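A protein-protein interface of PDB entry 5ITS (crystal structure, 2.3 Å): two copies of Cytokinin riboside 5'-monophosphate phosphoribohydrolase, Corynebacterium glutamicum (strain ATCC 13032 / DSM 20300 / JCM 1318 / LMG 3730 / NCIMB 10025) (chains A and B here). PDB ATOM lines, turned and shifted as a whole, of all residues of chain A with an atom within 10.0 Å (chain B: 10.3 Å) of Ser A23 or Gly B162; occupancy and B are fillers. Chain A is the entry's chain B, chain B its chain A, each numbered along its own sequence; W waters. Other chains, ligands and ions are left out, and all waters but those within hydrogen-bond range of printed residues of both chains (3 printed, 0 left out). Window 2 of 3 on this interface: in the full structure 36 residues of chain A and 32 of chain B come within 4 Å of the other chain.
The backbone carbonyl oxygen (O) of Arg B161 is in hydrogen-bond range of the backbone NH (N) of Ser A23 (3.0 Å).
OH of Tyr A27 sits at hydrogen-bond distance from NE of Arg B161, 3.2 Å away.
NH2 of Arg B161 lies within hydrogen-bond range of O of Asp A145.
The side-chain sulfur of Met B158 lies close to the backbone carbonyl oxygen of Gly A115 (3.8 Å).
O of Met B158 is in hydrogen-bond range of N of Phe B163, at 3.0 Å.
N of Leu A54 lies within hydrogen-bond range of O of Gly A18 (3.4 Å).
The backbone carbonyl oxygen (O) of Pro A114 lies within hydrogen-bond range of the backbone NH (N) of Gly A18.
The backbone carbonyl oxygen of Ala A20 lies within hydrogen-bond range of the backbone NH of Leu A54 (3.3 Å).
Water W3 lies within hydrogen-bond range of the backbone carbonyl oxygen of Gln B160 and the side-chain hydroxyl of Ser A23.
Water W1 lies within hydrogen-bond range of O of Phe B163, N of Ala A117 and OE1 of Gln B131.
Water W2 lies within hydrogen-bond range of the backbone carbonyl oxygen (O) of Phe B163 (3.3 Å) and the backbone NH (N) of Gly A116 (3.4 Å).
Printed residues of chain B within 4 Å of Ala A20: Gly B162 and Phe B163.
Of chain B, only Arg B161 (3.5 Å) and Phe B163 (3.5 Å) come within 4 Å of Gly A22.
Ser A23 touches two residues of chain B.
No residue of chain B comes within 4 Å of Ser A24.
Printed residues of chain B within 4 Å of Leu A54: Phe B163 (3.97 Å).
Printed residues of chain B within 4 Å of Asp A145: Arg B161 (3.3 Å).
Met B154 touches none of the printed residues of chain A.
Printed residues of chain A within 4 Å of Met B158: Gly A115 (3.8 Å).
Of the printed residues of chain A, Gly B162 touches Ala A20 (3.996 Å) and Ser A23 (3.6 Å).
Phe B163 touches just these residues of chain A: Ala A20 (3.5 Å), Leu A21 (3.9 Å), Gly A22 (3.5 Å), Tyr A27 (3.7 Å), Leu A54 (3.97 Å), Pro A114 (3.9 Å), Gly A115 (3.5 Å), Gly A116 (3.5 Å) and Phe A147 (3.5 Å).
The nearest printed residue of chain A that does not touch Gly B162 is Gly A22 (4.4 Å).
No position is printed for both chains.
Hydrophobic or aromatic side chains of chain B that line the printed part of chain A: Met B158 and Phe B163.
Hydrophobic or aromatic side chains of chain A that line the printed part of chain B: Ala A20, Tyr A27, Leu A54, Pro A114 and Phe A147.
Along chain A the printed residues that touch a printed residue of chain B span positions 20 to 147.
Among the printed residues, 17 pairs touch across the chains.
Among the printed residues, no Asp or Glu carboxylate lies within 4 Å of a Lys or Arg side-chain nitrogen of the other chain.
Among the printed residues, pairs that only touch across the chains: Ala A20 with Gly B162 (3.996 Å), Ala A20 with Phe B163 (3.5 Å), Leu A21 with Phe B163 (3.9 Å), Gly A22 with Arg B161 (3.5 Å), Gly A22 with Phe B163 (3.5 Å), Ser A23 with Gly B162 (3.6 Å), Tyr A27 with Phe B163 (3.7 Å), Leu A54 with Phe B163 (3.97 Å), Pro A114 with Phe B163 (3.9 Å), Gly A115 with Phe B163 (3.5 Å), Gly A116 with Phe B163 (3.5 Å), Phe A147 with Arg B161 (3.6 Å) and Phe A147 with Phe B163 (3.5 Å).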
ATOM      1  N   GLY A  18      19.143  -1.175  10.338  1.00  0.00           N
ATOM      2  CA  GLY A  18      20.567  -1.200   9.941  1.00  0.00           C
ATOM      3  C   GLY A  18      21.060  -2.573   9.534  1.00  0.00           C
ATOM      4  O   GLY A  18      20.468  -3.584   9.876  1.00  0.00           O
ATOM      5  N   SER A  19      22.158  -2.612   8.797  1.00  0.00           N
ATOM      6  CA  SER A  19      22.879  -3.889   8.597  1.00  0.00           C
ATOM      7  C   SER A  19      24.001  -4.095   9.632  1.00  0.00           C
ATOM      8  O   SER A  19      24.794  -5.032   9.505  1.00  0.00           O
ATOM      9  CB  SER A  19      23.484  -3.950   7.208  1.00  0.00           C
ATOM     10  OG  SER A  19      24.326  -2.825   6.996  1.00  0.00           O
ATOM     11  N   ALA A  20      24.077  -3.192  10.604  1.00  0.00           N
ATOM     12  CA  ALA A  20      24.846  -3.379  11.811  1.00  0.00           C
ATOM     13  C   ALA A  20      23.903  -3.620  12.983  1.00  0.00           C
ATOM     14  O   ALA A  20      22.751  -3.218  12.960  1.00  0.00           O
ATOM     15  CB  ALA A  20      25.652  -2.121  12.079  1.00  0.00           C
ATOM     16  N   LEU A  21      24.416  -4.226  14.042  1.00  0.00           N
ATOM     17  CA  LEU A  21      23.632  -4.429  15.255  1.00  0.00           C
ATOM     18  C   LEU A  21      23.581  -3.178  16.106  1.00  0.00           C
ATOM     19  O   LEU A  21      22.697  -3.037  16.937  1.00  0.00           O
ATOM     20  CB  LEU A  21      24.243  -5.562  16.101  1.00  0.00           C
ATOM     21  CG  LEU A  21      24.282  -6.962  15.473  1.00  0.00           C
ATOM     22  CD1 LEU A  21      25.135  -7.954  16.267  1.00  0.00           C
ATOM     23  CD2 LEU A  21      22.873  -7.470  15.316  1.00  0.00           C
ATOM     24  N   GLY A  22      24.531  -2.274  15.895  1.00  0.00           N
ATOM     25  CA  GLY A  22      24.611  -1.088  16.695  1.00  0.00           C
ATOM     26  C   GLY A  22      25.211  -1.447  18.023  1.00  0.00           C
ATOM     27  O   GLY A  22      25.519  -2.595  18.245  1.00  0.00           O
ATOM     28  N   SER A  23      25.304  -0.456  18.905  1.00  0.00           N
ATOM     29  CA  SER A  23      26.101  -0.512  20.124  1.00  0.00           C
ATOM     30  C   SER A  23      25.337  -0.793  21.415  1.00  0.00           C
ATOM     31  O   SER A  23      25.881  -0.607  22.505  1.00  0.00           O
ATOM     32  CB  SER A  23      26.786   0.826  20.307  1.00  0.00           C
ATOM     33  OG  SER A  23      27.684   1.038  19.267  1.00  0.00           O
ATOM     34  N   SER A  24      24.089  -1.224  21.315  1.00  0.00           N
ATOM     35  CA  SER A  24      23.409  -1.752  22.497  1.00  0.00           C
ATOM     36  C   SER A  24      22.809  -3.109  22.184  1.00  0.00           C
ATOM     37  O   SER A  24      22.243  -3.315  21.093  1.00  0.00           O
ATOM     38  CB  SER A  24      22.306  -0.801  22.966  1.00  0.00           C
ATOM     39  OG  SER A  24      21.772  -1.257  24.200  1.00  0.00           O
ATOM     40  N   SER A  25      22.959  -4.044  23.118  1.00  0.00           N
ATOM     41  CA  SER A  25      22.219  -5.296  23.054  1.00  0.00           C
ATOM     42  C   SER A  25      20.706  -5.029  22.955  1.00  0.00           C
ATOM     43  O   SER A  25      19.988  -5.799  22.326  1.00  0.00           O
ATOM     44  CB  SER A  25      22.514  -6.192  24.271  1.00  0.00           C
ATOM     45  OG  SER A  25      23.668  -6.977  24.039  1.00  0.00           O
ATOM     46  N   LEU A  26      20.246  -3.946  23.564  1.00  0.00           N
ATOM     47  CA  LEU A  26      18.838  -3.550  23.540  1.00  0.00           C
ATOM     48  C   LEU A  26      18.152  -3.492  22.146  1.00  0.00           C
ATOM     49  O   LEU A  26      16.943  -3.745  22.020  1.00  0.00           O
ATOM     50  CB  LEU A  26      18.708  -2.193  24.235  1.00  0.00           C
ATOM     51  CG  LEU A  26      17.306  -1.638  24.476  1.00  0.00           C
ATOM     52  CD1 LEU A  26      16.434  -2.688  25.156  1.00  0.00           C
ATOM     53  CD2 LEU A  26      17.328  -0.369  25.326  1.00  0.00           C
ATOM     54  N   TYR A  27      18.898  -3.178  21.096  1.00  0.00           N
ATOM     55  CA  TYR A  27      18.282  -3.001  19.798  1.00  0.00           C
ATOM     56  C   TYR A  27      17.986  -4.350  19.204  1.00  0.00           C
ATOM     57  O   TYR A  27      17.105  -4.484  18.317  1.00  0.00           O
ATOM     58  CB  TYR A  27      19.239  -2.264  18.831  1.00  0.00           C
ATOM     59  CG  TYR A  27      19.726  -0.903  19.305  1.00  0.00           C
ATOM     60  CD1 TYR A  27      18.863  -0.015  19.903  1.00  0.00           C
ATOM     61  CD2 TYR A  27      21.052  -0.507  19.119  1.00  0.00           C
ATOM     62  CE1 TYR A  27      19.316   1.222  20.359  1.00  0.00           C
ATOM     63  CE2 TYR A  27      21.519   0.742  19.550  1.00  0.00           C
ATOM     64  CZ  TYR A  27      20.650   1.608  20.166  1.00  0.00           C
ATOM     65  OH  TYR A  27      21.063   2.853  20.616  1.00  0.00           O
ATOM     66  N   THR A  28      18.793  -5.342  19.595  1.00  0.00           N
ATOM     67  CA  THR A  28      18.546  -6.709  19.202  1.00  0.00           C
ATOM     68  C   THR A  28      17.319  -7.216  19.966  1.00  0.00           C
ATOM     69  O   THR A  28      16.348  -7.657  19.375  1.00  0.00           O
ATOM     70  CB  THR A  28      19.784  -7.592  19.418  1.00  0.00           C
ATOM     71  OG1 THR A  28      20.818  -7.199  18.510  1.00  0.00           O
ATOM     72  CG2 THR A  28      19.457  -9.070  19.156  1.00  0.00           C
ATOM     73  N   GLY A  53      23.316  -7.972  11.297  1.00  0.00           N
ATOM     74  CA  GLY A  53      22.818  -6.781  11.954  1.00  0.00           C
ATOM     75  C   GLY A  53      21.345  -6.875  12.276  1.00  0.00           C
ATOM     76  O   GLY A  53      20.802  -7.942  12.333  1.00  0.00           O
ATOM     77  N   LEU A  54      20.707  -5.739  12.476  1.00  0.00           N
ATOM     78  CA  LEU A  54      19.306  -5.721  12.836  1.00  0.00           C
ATOM     79  C   LEU A  54      18.426  -6.263  11.703  1.00  0.00           C
ATOM     80  O   LEU A  54      17.451  -6.934  11.946  1.00  0.00           O
ATOM     81  CB  LEU A  54      18.882  -4.318  13.237  1.00  0.00           C
ATOM     82  CG  LEU A  54      19.586  -3.721  14.475  1.00  0.00           C
ATOM     83  CD1 LEU A  54      18.990  -2.397  14.924  1.00  0.00           C
ATOM     84  CD2 LEU A  54      19.544  -4.724  15.593  1.00  0.00           C
ATOM     85  N   PRO A 114      16.101   1.261  14.566  1.00  0.00           N
ATOM     86  CA  PRO A 114      17.380   1.924  14.526  1.00  0.00           C
ATOM     87  C   PRO A 114      18.254   1.491  13.386  1.00  0.00           C
ATOM     88  O   PRO A 114      18.290   0.364  13.053  1.00  0.00           O
ATOM     89  CB  PRO A 114      17.947   1.603  15.866  1.00  0.00           C
ATOM     90  CG  PRO A 114      16.778   1.713  16.716  1.00  0.00           C
ATOM     91  CD  PRO A 114      15.671   1.095  15.951  1.00  0.00           C
ATOM     92  N   GLY A 115      18.909   2.455  12.785  1.00  0.00           N
ATOM     93  CA  GLY A 115      19.820   2.210  11.685  1.00  0.00           C
ATOM     94  C   GLY A 115      20.532   3.480  11.312  1.00  0.00           C
ATOM     95  O   GLY A 115      20.454   4.519  12.000  1.00  0.00           O
ATOM     96  N   GLY A 116      21.240   3.422  10.213  1.00  0.00           N
ATOM     97  CA  GLY A 116      21.953   4.568   9.768  1.00  0.00           C
ATOM     98  C   GLY A 116      21.372   5.269   8.576  1.00  0.00           C
ATOM     99  O   GLY A 116      20.185   5.389   8.425  1.00  0.00           O
ATOM    100  N   ALA A 117      22.269   5.738   7.725  1.00  0.00           N
ATOM    101  CA  ALA A 117      21.936   6.504   6.532  1.00  0.00           C
ATOM    102  C   ALA A 117      20.879   5.855   5.668  1.00  0.00           C
ATOM    103  O   ALA A 117      19.893   6.520   5.260  1.00  0.00           O
ATOM    104  CB  ALA A 117      23.199   6.706   5.692  1.00  0.00           C
ATOM    105  N   VAL A 144      13.224   3.005  20.106  1.00  0.00           N
ATOM    106  CA  VAL A 144      13.883   2.150  21.042  1.00  0.00           C
ATOM    107  C   VAL A 144      14.853   2.985  21.816  1.00  0.00           C
ATOM    108  O   VAL A 144      15.736   3.589  21.237  1.00  0.00           O
ATOM    109  CB  VAL A 144      14.693   1.067  20.306  1.00  0.00           C
ATOM    110  CG1 VAL A 144      15.440   0.211  21.291  1.00  0.00           C
ATOM    111  CG2 VAL A 144      13.787   0.190  19.497  1.00  0.00           C
ATOM    112  N   ASP A 145      14.707   2.998  23.128  1.00  0.00           N
ATOM    113  CA  ASP A 145      15.496   3.845  24.009  1.00  0.00           C
ATOM    114  C   ASP A 145      15.684   5.276  23.478  1.00  0.00           C
ATOM    115  O   ASP A 145      16.781   5.844  23.582  1.00  0.00           O
ATOM    116  CB  ASP A 145      16.858   3.194  24.321  1.00  0.00           C
ATOM    117  CG  ASP A 145      17.567   3.830  25.556  1.00  0.00           C
ATOM    118  OD1 ASP A 145      16.910   4.163  26.618  1.00  0.00           O
ATOM    119  OD2 ASP A 145      18.802   3.996  25.438  1.00  0.00           O
ATOM    120  N   PHE A 147      15.850   6.473  20.534  1.00  0.00           N
ATOM    121  CA  PHE A 147      16.849   6.562  19.454  1.00  0.00           C
ATOM    122  C   PHE A 147      16.495   7.648  18.444  1.00  0.00           C
ATOM    123  O   PHE A 147      17.358   8.375  17.971  1.00  0.00           O
ATOM    124  CB  PHE A 147      16.871   5.231  18.724  1.00  0.00           C
ATOM    125  CG  PHE A 147      17.876   5.155  17.633  1.00  0.00           C
ATOM    126  CD1 PHE A 147      19.163   4.711  17.897  1.00  0.00           C
ATOM    127  CD2 PHE A 147      17.543   5.504  16.360  1.00  0.00           C
ATOM    128  CE1 PHE A 147      20.099   4.594  16.892  1.00  0.00           C
ATOM    129  CE2 PHE A 147      18.472   5.416  15.340  1.00  0.00           C
ATOM    130  CZ  PHE A 147      19.755   4.954  15.599  1.00  0.00           C
ATOM    131  N   GLN B 131      28.255   6.176   0.268  1.00  0.00           N
ATOM    132  CA  GLN B 131      28.795   5.210   1.213  1.00  0.00           C
ATOM    133  C   GLN B 131      29.004   3.857   0.558  1.00  0.00           C
ATOM    134  O   GLN B 131      29.957   3.197   0.863  1.00  0.00           O
ATOM    135  CB  GLN B 131      27.895   5.007   2.425  1.00  0.00           C
ATOM    136  CG  GLN B 131      28.572   4.169   3.510  1.00  0.00           C
ATOM    137  CD  GLN B 131      27.934   4.372   4.902  1.00  0.00           C
ATOM    138  OE1 GLN B 131      26.718   4.685   5.012  1.00  0.00           O
ATOM    139  NE2 GLN B 131      28.756   4.192   5.985  1.00  0.00           N
ATOM    140  N   MET B 154      21.844  14.614  14.917  1.00  0.00           N
ATOM    141  CA  MET B 154      21.230  13.328  14.754  1.00  0.00           C
ATOM    142  C   MET B 154      22.263  12.388  14.183  1.00  0.00           C
ATOM    143  O   MET B 154      22.443  11.321  14.693  1.00  0.00           O
ATOM    144  CB  MET B 154      20.064  13.432  13.838  1.00  0.00           C
ATOM    145  CG  MET B 154      19.360  12.116  13.598  1.00  0.00           C
ATOM    146  SD  MET B 154      18.224  12.275  12.200  1.00  0.00           S
ATOM    147  CE  MET B 154      19.375  12.645  10.857  1.00  0.00           C
ATOM    148  N   LEU B 155      22.942  12.788  13.128  1.00  0.00           N
ATOM    149  CA  LEU B 155      23.980  11.945  12.587  1.00  0.00           C
ATOM    150  C   LEU B 155      25.101  11.655  13.615  1.00  0.00           C
ATOM    151  O   LEU B 155      25.668  10.550  13.664  1.00  0.00           O
ATOM    152  CB  LEU B 155      24.570  12.615  11.354  1.00  0.00           C
ATOM    153  CG  LEU B 155      23.570  12.723  10.195  1.00  0.00           C
ATOM    154  CD1 LEU B 155      24.288  13.198   8.957  1.00  0.00           C
ATOM    155  CD2 LEU B 155      22.883  11.413   9.905  1.00  0.00           C
ATOM    156  N   GLU B 156      25.383  12.621  14.483  1.00  0.00           N
ATOM    157  CA  GLU B 156      26.458  12.422  15.427  1.00  0.00           C
ATOM    158  C   GLU B 156      26.080  11.293  16.392  1.00  0.00           C
ATOM    159  O   GLU B 156      26.884  10.412  16.671  1.00  0.00           O
ATOM    160  CB  GLU B 156      26.811  13.736  16.124  1.00  0.00           C
ATOM    161  CG  GLU B 156      27.807  13.614  17.293  1.00  0.00           C
ATOM    162  CD  GLU B 156      29.230  13.212  16.892  1.00  0.00           C
ATOM    163  OE1 GLU B 156      29.939  12.540  17.707  1.00  0.00           O
ATOM    164  OE2 GLU B 156      29.631  13.546  15.748  1.00  0.00           O
ATOM    165  N   GLN B 157      24.836  11.280  16.844  1.00  0.00           N
ATOM    166  CA  GLN B 157      24.373  10.240  17.716  1.00  0.00           C
ATOM    167  C   GLN B 157      24.330   8.901  17.009  1.00  0.00           C
ATOM    168  O   GLN B 157      24.665   7.889  17.597  1.00  0.00           O
ATOM    169  CB  GLN B 157      22.981  10.552  18.171  1.00  0.00           C
ATOM    170  CG  GLN B 157      22.879  11.856  18.905  1.00  0.00           C
ATOM    171  CD  GLN B 157      23.379  11.718  20.291  1.00  0.00           C
ATOM    172  OE1 GLN B 157      22.681  11.173  21.149  1.00  0.00           O
ATOM    173  NE2 GLN B 157      24.612  12.169  20.530  1.00  0.00           N
ATOM    174  N   MET B 158      23.911   8.864  15.752  1.00  0.00           N
ATOM    175  CA  MET B 158      23.893   7.583  15.073  1.00  0.00           C
ATOM    176  C   MET B 158      25.304   7.027  14.992  1.00  0.00           C
ATOM    177  O   MET B 158      25.497   5.848  15.150  1.00  0.00           O
ATOM    178  CB  MET B 158      23.288   7.683  13.704  1.00  0.00           C
ATOM    179  CG  MET B 158      21.819   7.964  13.821  1.00  0.00           C
ATOM    180  SD  MET B 158      21.122   8.210  12.167  1.00  0.00           S
ATOM    181  CE  MET B 158      19.485   8.612  12.760  1.00  0.00           C
ATOM    182  N   THR B 159      26.273   7.894  14.770  1.00  0.00           N
ATOM    183  CA  THR B 159      27.656   7.471  14.677  1.00  0.00           C
ATOM    184  C   THR B 159      28.121   6.956  16.042  1.00  0.00           C
ATOM    185  O   THR B 159      28.735   5.906  16.137  1.00  0.00           O
ATOM    186  CB  THR B 159      28.533   8.624  14.182  1.00  0.00           C
ATOM    187  OG1 THR B 159      28.024   9.109  12.907  1.00  0.00           O
ATOM    188  CG2 THR B 159      29.956   8.148  14.017  1.00  0.00           C
ATOM    189  N   GLN B 160      27.708   7.622  17.102  1.00  0.00           N
ATOM    190  CA  GLN B 160      28.058   7.171  18.427  1.00  0.00           C
ATOM    191  C   GLN B 160      27.321   5.908  18.865  1.00  0.00           C
ATOM    192  O   GLN B 160      27.725   5.265  19.835  1.00  0.00           O
ATOM    193  CB  GLN B 160      27.831   8.271  19.450  1.00  0.00           C
ATOM    194  CG  GLN B 160      28.912   9.324  19.389  1.00  0.00           C
ATOM    195  CD  GLN B 160      28.713  10.449  20.374  1.00  0.00           C
ATOM    196  OE1 GLN B 160      28.125  10.277  21.415  1.00  0.00           O
ATOM    197  NE2 GLN B 160      29.186  11.610  20.023  1.00  0.00           N
ATOM    198  N   ARG B 161      26.235   5.562  18.192  1.00  0.00           N
ATOM    199  CA  ARG B 161      25.517   4.353  18.530  1.00  0.00           C
ATOM    200  C   ARG B 161      25.832   3.238  17.545  1.00  0.00           C
ATOM    201  O   ARG B 161      25.192   2.223  17.597  1.00  0.00           O
ATOM    202  CB  ARG B 161      24.008   4.614  18.703  1.00  0.00           C
ATOM    203  CG  ARG B 161      23.708   5.276  20.040  1.00  0.00           C
ATOM    204  CD  ARG B 161      22.734   6.446  19.943  1.00  0.00           C
ATOM    205  NE  ARG B 161      21.380   6.074  20.333  1.00  0.00           N
ATOM    206  CZ  ARG B 161      20.788   6.441  21.466  1.00  0.00           C
ATOM    207  NH1 ARG B 161      21.430   7.229  22.336  1.00  0.00           N
ATOM    208  NH2 ARG B 161      19.548   6.007  21.740  1.00  0.00           N
ATOM    209  N   GLY B 162      26.838   3.399  16.690  1.00  0.00           N
ATOM    210  CA  GLY B 162      27.314   2.272  15.876  1.00  0.00           C
ATOM    211  C   GLY B 162      26.748   2.124  14.466  1.00  0.00           C
ATOM    212  O   GLY B 162      27.153   1.197  13.725  1.00  0.00           O
ATOM    213  N   PHE B 163      25.866   3.035  14.033  1.00  0.00           N
ATOM    214  CA  PHE B 163      25.168   2.820  12.759  1.00  0.00           C
ATOM    215  C   PHE B 163      25.703   3.590  11.577  1.00  0.00           C
ATOM    216  O   PHE B 163      25.237   3.431  10.446  1.00  0.00           O
ATOM    217  CB  PHE B 163      23.680   3.079  12.895  1.00  0.00           C
ATOM    218  CG  PHE B 163      22.993   2.147  13.827  1.00  0.00           C
ATOM    219  CD1 PHE B 163      22.790   0.822  13.471  1.00  0.00           C
ATOM    220  CD2 PHE B 163      22.548   2.596  15.058  1.00  0.00           C
ATOM    221  CE1 PHE B 163      22.151  -0.036  14.339  1.00  0.00           C
ATOM    222  CE2 PHE B 163      21.898   1.758  15.926  1.00  0.00           C
ATOM    223  CZ  PHE B 163      21.688   0.447  15.570  1.00  0.00           C
ATOM    224  N   ILE B 164      26.689   4.435  11.823  1.00  0.00           N
ATOM    225  CA  ILE B 164      27.329   5.153  10.721  1.00  0.00           C
ATOM    226  C   ILE B 164      28.817   5.149  10.928  1.00  0.00           C
ATOM    227  O   ILE B 164      29.297   5.492  11.987  1.00  0.00           O
ATOM    228  CB  ILE B 164      26.823   6.608  10.703  1.00  0.00           C
ATOM    229  CG1 ILE B 164      25.319   6.619  10.592  1.00  0.00           C
ATOM    230  CG2 ILE B 164      27.421   7.388   9.555  1.00  0.00           C
ATOM    231  CD1 ILE B 164      24.757   7.990  10.344  1.00  0.00           C
ATOM    232  N   LYS B 165      29.553   4.813   9.903  1.00  0.00           N
ATOM    233  CA  LYS B 165      31.000   4.854  10.008  1.00  0.00           C
ATOM    234  C   LYS B 165      31.455   6.283  10.156  1.00  0.00           C
ATOM    235  O   LYS B 165      31.052   7.133   9.360  1.00  0.00           O
ATOM    236  CB  LYS B 165      31.653   4.177   8.808  1.00  0.00           C
ATOM    237  CG  LYS B 165      31.181   2.719   8.694  1.00  0.00           C
ATOM    238  CD  LYS B 165      32.287   1.716   8.286  1.00  0.00           C
ATOM    239  CE  LYS B 165      32.042   0.289   8.842  1.00  0.00           C
ATOM    240  NZ  LYS B 165      33.222  -0.633   8.717  1.00  0.00           N
ATOM    241  N   ARG B 166      32.256   6.551  11.194  1.00  0.00           N
ATOM    242  CA  ARG B 166      32.730   7.921  11.528  1.00  0.00           C
ATOM    243  C   ARG B 166      33.495   8.546  10.379  1.00  0.00           C
ATOM    244  O   ARG B 166      33.433   9.772  10.145  1.00  0.00           O
ATOM    245  CB  ARG B 166      33.647   7.896  12.763  1.00  0.00           C
ATOM    246  CG  ARG B 166      34.567   9.103  12.971  1.00  0.00           C
ATOM    247  CD  ARG B 166      33.751  10.299  13.391  1.00  0.00           C
ATOM    248  NE  ARG B 166      33.064  10.060  14.643  1.00  0.00           N
ATOM    249  CZ  ARG B 166      32.103  10.846  15.128  1.00  0.00           C
ATOM    250  NH1 ARG B 166      31.695  11.881  14.434  1.00  0.00           N
ATOM    251  NH2 ARG B 166      31.535  10.618  16.328  1.00  0.00           N
HETATM  252  O   HOH W   1      24.860   4.363   7.730  1.00  0.00           O
HETATM  253  O   HOH W   2      23.380   0.725  10.355  1.00  0.00           O
HETATM  254  O   HOH W   3      29.574   3.160  19.646  1.00  0.00           O
